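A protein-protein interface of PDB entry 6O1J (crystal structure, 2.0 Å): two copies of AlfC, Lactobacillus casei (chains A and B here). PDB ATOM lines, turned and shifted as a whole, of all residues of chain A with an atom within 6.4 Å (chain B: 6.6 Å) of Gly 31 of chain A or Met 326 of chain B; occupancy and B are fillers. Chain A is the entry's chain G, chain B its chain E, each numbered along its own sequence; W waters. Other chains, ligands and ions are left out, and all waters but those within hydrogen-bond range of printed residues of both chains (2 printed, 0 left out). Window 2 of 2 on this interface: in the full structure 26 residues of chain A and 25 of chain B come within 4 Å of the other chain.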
ATOM      1  N   GLY A  27      -8.635   4.859   0.527  1.00  0.00           N
ATOM      2  CA  GLY A  27      -7.175   4.726   0.357  1.00  0.00           C
ATOM      3  C   GLY A  27      -6.712   3.291   0.361  1.00  0.00           C
ATOM      4  O   GLY A  27      -5.516   3.068   0.422  1.00  0.00           O
ATOM      5  N   GLU A  28      -7.645   2.350   0.234  1.00  0.00           N
ATOM      6  CA  GLU A  28      -7.415   0.899   0.354  1.00  0.00           C
ATOM      7  C   GLU A  28      -8.208   0.173  -0.741  1.00  0.00           C
ATOM      8  O   GLU A  28      -9.370   0.499  -0.922  1.00  0.00           O
ATOM      9  CB  GLU A  28      -7.894   0.481   1.738  1.00  0.00           C
ATOM     10  CG  GLU A  28      -7.211  -0.753   2.271  1.00  0.00           C
ATOM     11  CD  GLU A  28      -7.838  -1.475   3.443  1.00  0.00           C
ATOM     12  OE1 GLU A  28      -8.754  -2.405   3.246  1.00  0.00           O
ATOM     13  OE2 GLU A  28      -7.357  -1.224   4.558  1.00  0.00           O
ATOM     14  N   TYR A  29      -7.592  -0.784  -1.422  1.00  0.00           N
ATOM     15  CA  TYR A  29      -8.258  -1.679  -2.387  1.00  0.00           C
ATOM     16  C   TYR A  29      -7.684  -3.086  -2.296  1.00  0.00           C
ATOM     17  O   TYR A  29      -6.490  -3.273  -2.560  1.00  0.00           O
ATOM     18  CB  TYR A  29      -8.134  -1.098  -3.796  1.00  0.00           C
ATOM     19  CG  TYR A  29      -8.878  -1.901  -4.821  1.00  0.00           C
ATOM     20  CD1 TYR A  29     -10.260  -1.846  -4.874  1.00  0.00           C
ATOM     21  CD2 TYR A  29      -8.218  -2.781  -5.672  1.00  0.00           C
ATOM     22  CE1 TYR A  29     -10.980  -2.592  -5.788  1.00  0.00           C
ATOM     23  CE2 TYR A  29      -8.920  -3.532  -6.598  1.00  0.00           C
ATOM     24  CZ  TYR A  29     -10.307  -3.430  -6.657  1.00  0.00           C
ATOM     25  OH  TYR A  29     -11.017  -4.162  -7.537  1.00  0.00           O
ATOM     26  N   ARG A  30      -8.547  -4.057  -1.958  1.00  0.00           N
ATOM     27  CA  ARG A  30      -8.232  -5.507  -1.869  1.00  0.00           C
ATOM     28  C   ARG A  30      -6.903  -5.696  -1.137  1.00  0.00           C
ATOM     29  O   ARG A  30      -6.019  -6.370  -1.671  1.00  0.00           O
ATOM     30  CB  ARG A  30      -8.217  -6.116  -3.275  1.00  0.00           C
ATOM     31  CG  ARG A  30      -9.563  -6.056  -3.979  1.00  0.00           C
ATOM     32  CD  ARG A  30      -9.579  -6.893  -5.237  1.00  0.00           C
ATOM     33  NE  ARG A  30     -10.826  -6.748  -5.972  1.00  0.00           N
ATOM     34  CZ  ARG A  30     -11.959  -7.422  -5.722  1.00  0.00           C
ATOM     35  NH1 ARG A  30     -12.036  -8.298  -4.736  1.00  0.00           N
ATOM     36  NH2 ARG A  30     -13.028  -7.203  -6.464  1.00  0.00           N
ATOM     37  N   GLY A  31      -6.788  -5.090   0.039  1.00  0.00           N
ATOM     38  CA  GLY A  31      -5.654  -5.269   0.954  1.00  0.00           C
ATOM     39  C   GLY A  31      -4.435  -4.441   0.580  1.00  0.00           C
ATOM     40  O   GLY A  31      -3.409  -4.678   1.190  1.00  0.00           O
ATOM     41  N   GLU A  32      -4.525  -3.516  -0.378  1.00  0.00           N
ATOM     42  CA  GLU A  32      -3.349  -2.707  -0.800  1.00  0.00           C
ATOM     43  C   GLU A  32      -3.655  -1.214  -0.725  1.00  0.00           C
ATOM     44  O   GLU A  32      -4.823  -0.809  -0.760  1.00  0.00           O
ATOM     45  CB  GLU A  32      -2.911  -3.162  -2.193  1.00  0.00           C
ATOM     46  CG  GLU A  32      -2.241  -4.516  -2.117  1.00  0.00           C
ATOM     47  CD  GLU A  32      -2.000  -5.185  -3.446  1.00  0.00           C
ATOM     48  OE1 GLU A  32      -2.564  -4.728  -4.482  1.00  0.00           O
ATOM     49  OE2 GLU A  32      -1.252  -6.165  -3.439  1.00  0.00           O
ATOM     50  N   SER A  33      -2.598  -0.430  -0.589  1.00  0.00           N
ATOM     51  CA  SER A  33      -2.659   1.015  -0.315  1.00  0.00           C
ATOM     52  C   SER A  33      -2.757   1.774  -1.642  1.00  0.00           C
ATOM     53  O   SER A  33      -2.080   1.392  -2.592  1.00  0.00           O
ATOM     54  CB  SER A  33      -1.479   1.463   0.486  1.00  0.00           C
ATOM     55  OG  SER A  33      -1.597   2.852   0.726  1.00  0.00           O
ATOM     56  N   SER A  34      -3.589   2.805  -1.694  1.00  0.00           N
ATOM     57  CA  SER A  34      -3.467   3.911  -2.682  1.00  0.00           C
ATOM     58  C   SER A  34      -2.043   4.481  -2.617  1.00  0.00           C
ATOM     59  O   SER A  34      -1.289   4.168  -1.663  1.00  0.00           O
ATOM     60  CB  SER A  34      -4.499   4.966  -2.442  1.00  0.00           C
ATOM     61  OG  SER A  34      -4.249   5.665  -1.231  1.00  0.00           O
ATOM     62  N   TYR A 287      -8.194   6.336   5.094  1.00  0.00           N
ATOM     63  CA  TYR A 287      -8.234   6.048   6.549  1.00  0.00           C
ATOM     64  C   TYR A 287      -6.793   5.783   7.024  1.00  0.00           C
ATOM     65  O   TYR A 287      -6.576   6.213   8.154  1.00  0.00           O
ATOM     66  CB  TYR A 287      -9.390   5.120   6.885  1.00  0.00           C
ATOM     67  CG  TYR A 287      -8.964   3.699   6.967  1.00  0.00           C
ATOM     68  CD1 TYR A 287      -8.268   3.257   8.083  1.00  0.00           C
ATOM     69  CD2 TYR A 287      -9.364   2.752   6.035  1.00  0.00           C
ATOM     70  CE1 TYR A 287      -7.887   1.928   8.221  1.00  0.00           C
ATOM     71  CE2 TYR A 287      -8.975   1.422   6.141  1.00  0.00           C
ATOM     72  CZ  TYR A 287      -8.272   1.001   7.260  1.00  0.00           C
ATOM     73  OH  TYR A 287      -7.880  -0.288   7.365  1.00  0.00           O
ATOM     74  N   HIS A 288      -5.865   5.299   6.193  1.00  0.00           N
ATOM     75  CA  HIS A 288      -4.496   4.941   6.625  1.00  0.00           C
ATOM     76  C   HIS A 288      -3.615   6.201   6.796  1.00  0.00           C
ATOM     77  O   HIS A 288      -2.629   6.118   7.524  1.00  0.00           O
ATOM     78  CB  HIS A 288      -3.815   3.906   5.729  1.00  0.00           C
ATOM     79  CG  HIS A 288      -3.479   4.319   4.347  1.00  0.00           C
ATOM     80  ND1 HIS A 288      -2.239   4.901   4.012  1.00  0.00           N
ATOM     81  CD2 HIS A 288      -4.168   4.197   3.186  1.00  0.00           C
ATOM     82  CE1 HIS A 288      -2.192   5.118   2.705  1.00  0.00           C
ATOM     83  NE2 HIS A 288      -3.382   4.692   2.165  1.00  0.00           N
ATOM     84  N   TRP B 292      -1.707  -0.851  15.747  1.00  0.00           N
ATOM     85  CA  TRP B 292      -1.666  -2.269  15.341  1.00  0.00           C
ATOM     86  C   TRP B 292      -0.525  -2.965  16.087  1.00  0.00           C
ATOM     87  O   TRP B 292       0.642  -2.485  15.998  1.00  0.00           O
ATOM     88  CB  TRP B 292      -1.491  -2.361  13.819  1.00  0.00           C
ATOM     89  CG  TRP B 292      -2.577  -1.663  13.047  1.00  0.00           C
ATOM     90  CD1 TRP B 292      -2.429  -0.518  12.337  1.00  0.00           C
ATOM     91  CD2 TRP B 292      -3.950  -2.071  12.866  1.00  0.00           C
ATOM     92  NE1 TRP B 292      -3.611  -0.174  11.740  1.00  0.00           N
ATOM     93  CE2 TRP B 292      -4.568  -1.099  12.055  1.00  0.00           C
ATOM     94  CE3 TRP B 292      -4.712  -3.156  13.309  1.00  0.00           C
ATOM     95  CZ2 TRP B 292      -5.910  -1.189  11.662  1.00  0.00           C
ATOM     96  CZ3 TRP B 292      -6.036  -3.254  12.932  1.00  0.00           C
ATOM     97  CH2 TRP B 292      -6.631  -2.267  12.140  1.00  0.00           C
ATOM     98  N   ARG B 323     -14.430  -5.308   4.797  1.00  0.00           N
ATOM     99  CA  ARG B 323     -13.025  -5.687   4.512  1.00  0.00           C
ATOM    100  C   ARG B 323     -12.270  -5.878   5.826  1.00  0.00           C
ATOM    101  O   ARG B 323     -12.515  -5.127   6.798  1.00  0.00           O
ATOM    102  CB  ARG B 323     -12.308  -4.617   3.662  1.00  0.00           C
ATOM    103  CG  ARG B 323     -12.945  -4.378   2.299  1.00  0.00           C
ATOM    104  CD  ARG B 323     -12.374  -3.252   1.475  1.00  0.00           C
ATOM    105  NE  ARG B 323     -12.293  -1.965   2.177  1.00  0.00           N
ATOM    106  CZ  ARG B 323     -11.827  -0.852   1.624  1.00  0.00           C
ATOM    107  NH1 ARG B 323     -11.418  -0.875   0.364  1.00  0.00           N
ATOM    108  NH2 ARG B 323     -11.771   0.269   2.319  1.00  0.00           N
ATOM    109  N   VAL B 324     -11.331  -6.814   5.817  1.00  0.00           N
ATOM    110  CA  VAL B 324     -10.226  -6.906   6.798  1.00  0.00           C
ATOM    111  C   VAL B 324      -9.327  -5.690   6.551  1.00  0.00           C
ATOM    112  O   VAL B 324      -8.832  -5.491   5.453  1.00  0.00           O
ATOM    113  CB  VAL B 324      -9.438  -8.214   6.670  1.00  0.00           C
ATOM    114  CG1 VAL B 324      -8.282  -8.251   7.691  1.00  0.00           C
ATOM    115  CG2 VAL B 324     -10.331  -9.436   6.811  1.00  0.00           C
ATOM    116  N   PRO B 325      -9.119  -4.801   7.542  1.00  0.00           N
ATOM    117  CA  PRO B 325      -8.217  -3.678   7.343  1.00  0.00           C
ATOM    118  C   PRO B 325      -6.860  -4.153   6.804  1.00  0.00           C
ATOM    119  O   PRO B 325      -6.349  -5.173   7.260  1.00  0.00           O
ATOM    120  CB  PRO B 325      -8.098  -3.074   8.740  1.00  0.00           C
ATOM    121  CG  PRO B 325      -9.340  -3.487   9.457  1.00  0.00           C
ATOM    122  CD  PRO B 325      -9.735  -4.816   8.874  1.00  0.00           C
ATOM    123  N   MET B 326      -6.298  -3.403   5.861  1.00  0.00           N
ATOM    124  CA  MET B 326      -4.977  -3.682   5.232  1.00  0.00           C
ATOM    125  C   MET B 326      -3.947  -4.031   6.310  1.00  0.00           C
ATOM    126  O   MET B 326      -3.211  -5.004   6.115  1.00  0.00           O
ATOM    127  CB  MET B 326      -4.494  -2.447   4.464  1.00  0.00           C
ATOM    128  CG  MET B 326      -3.086  -2.556   3.918  1.00  0.00           C
ATOM    129  SD  MET B 326      -2.755  -1.132   2.822  1.00  0.00           S
ATOM    130  CE  MET B 326      -3.564   0.260   3.610  1.00  0.00           C
ATOM    131  N   MET B 327      -3.875  -3.269   7.400  1.00  0.00           N
ATOM    132  CA  MET B 327      -2.791  -3.478   8.394  1.00  0.00           C
ATOM    133  C   MET B 327      -3.106  -4.711   9.259  1.00  0.00           C
ATOM    134  O   MET B 327      -2.139  -5.382   9.622  1.00  0.00           O
ATOM    135  CB  MET B 327      -2.539  -2.232   9.238  1.00  0.00           C
ATOM    136  CG  MET B 327      -1.658  -1.190   8.533  1.00  0.00           C
ATOM    137  SD  MET B 327      -0.186  -1.954   7.732  1.00  0.00           S
ATOM    138  CE  MET B 327       0.717  -2.584   9.134  1.00  0.00           C
ATOM    139  N   ALA B 328      -4.391  -5.012   9.544  1.00  0.00           N
ATOM    140  CA  ALA B 328      -4.785  -6.252  10.250  1.00  0.00           C
ATOM    141  C   ALA B 328      -4.311  -7.462   9.435  1.00  0.00           C
ATOM    142  O   ALA B 328      -3.613  -8.321   9.998  1.00  0.00           O
ATOM    143  CB  ALA B 328      -6.273  -6.311  10.500  1.00  0.00           C
ATOM    144  N   GLU B 329      -4.576  -7.456   8.126  1.00  0.00           N
ATOM    145  CA  GLU B 329      -4.193  -8.554   7.211  1.00  0.00           C
ATOM    146  C   GLU B 329      -2.669  -8.659   7.110  1.00  0.00           C
ATOM    147  O   GLU B 329      -2.178  -9.805   7.169  1.00  0.00           O
ATOM    148  CB  GLU B 329      -4.797  -8.342   5.824  1.00  0.00           C
ATOM    149  CG  GLU B 329      -4.339  -9.377   4.827  1.00  0.00           C
ATOM    150  CD  GLU B 329      -5.218  -9.578   3.611  1.00  0.00           C
ATOM    151  OE1 GLU B 329      -6.099  -8.745   3.355  1.00  0.00           O
ATOM    152  OE2 GLU B 329      -5.023 -10.551   2.937  1.00  0.00           O
ATOM    153  N   GLU B 330      -1.942  -7.537   6.930  1.00  0.00           N
ATOM    154  CA  GLU B 330      -0.463  -7.593   6.798  1.00  0.00           C
ATOM    155  C   GLU B 330       0.148  -8.149   8.075  1.00  0.00           C
ATOM    156  O   GLU B 330       1.086  -8.958   7.972  1.00  0.00           O
ATOM    157  CB  GLU B 330       0.164  -6.235   6.556  1.00  0.00           C
ATOM    158  CG  GLU B 330       0.034  -5.720   5.134  1.00  0.00           C
ATOM    159  CD  GLU B 330       0.991  -4.556   4.835  1.00  0.00           C
ATOM    160  OE1 GLU B 330       2.100  -4.525   5.409  1.00  0.00           O
ATOM    161  OE2 GLU B 330       0.630  -3.671   4.074  1.00  0.00           O
ATOM    162  N   ASN B 331      -0.339  -7.721   9.235  1.00  0.00           N
ATOM    163  CA  ASN B 331       0.267  -8.109  10.531  1.00  0.00           C
ATOM    164  C   ASN B 331      -0.068  -9.568  10.831  1.00  0.00           C
ATOM    165  O   ASN B 331       0.827 -10.286  11.356  1.00  0.00           O
ATOM    166  CB  ASN B 331      -0.132  -7.134  11.646  1.00  0.00           C
ATOM    167  CG  ASN B 331       0.523  -5.772  11.522  1.00  0.00           C
ATOM    168  OD1 ASN B 331       1.101  -5.419  10.496  1.00  0.00           O
ATOM    169  ND2 ASN B 331       0.452  -5.008  12.585  1.00  0.00           N
HETATM  170  O   HOH W   1     -11.661  -3.420  -1.701  1.00  0.00           O
HETATM  171  O   HOH W   2      -5.306  -0.859   7.704  1.00  0.00           O
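Hydrophobic or aromatic side chains of chain B that line the printed part of chain A: Pro 325 and Met 326. Hydrophobic or aromatic side chains of chain A within 4 Å of the printed part of chain B: Tyr 287.
Gly 31 of chain A touches just one residue of chain B: Met 326. Of the printed residues of chain A, Pro 325 of chain B touches Glu 28 and Tyr 287. Of the printed residues of chain B, Glu 28 of chain A touches Arg 323 (2.8 Å), Val 324 (3.8 Å), Pro 325 (3.7 Å) and Met 326 (2.8 Å). The nearest printed residue of chain A that does not touch Met 326 of chain B is His 288 of chain A (4.01 Å).
The side-chain sulfur (SD) of Met 326 of chain B sits at hydrogen-bond distance from the backbone NH (N) of Ser 33 of chain A (3.5 Å). The side-chain carboxylate (OE1) of Glu 28 of chain A is in salt-bridge range of the guanidinium group (NE) of Arg 323 of chain B (3.7 Å). The backbone NH of Met 326 of chain B is in hydrogen-bond range of the side-chain carboxylate of Glu 28 of chain A, 2.8 Å away.
Among the printed residues, pairs that only touch across the chains: Tyr 287 of chain A with Pro 325 of chain B, Gly 31 of chain A with Met 326 of chain B, Glu 32 of chain A with Met 326 of chain B, Glu 28 of chain A with Pro 325 of chain B, Glu 28 of chain A with Val 324 of chain B and Tyr 287 of chain A with Met 326 of chain B.
No position is printed for both chains. Of the 9 pairs that touch across the chains among the printed residues, none has its exchanged pair printed and touching as well.
Water W2 lies within hydrogen-bond range of the side-chain hydroxyl (OH) of Tyr 287 of chain A (2.7 Å), the backbone NH (N) of Met 327 of chain B (2.8 Å) and the backbone NH (N) of Met 326 of chain B (3.3 Å). Water W1 bridges N of Arg 30 of chain A and NH1 of Arg 323 of chain B.
The side-chain carboxylate (OE2) of Glu 28 of chain A lies within hydrogen-bond range of the side-chain hydroxyl (OH) of Tyr 287 of chain A (3.0 Å). NE2 of His 288 of chain A lies within hydrogen-bond range of OG of Ser 33 of chain A.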
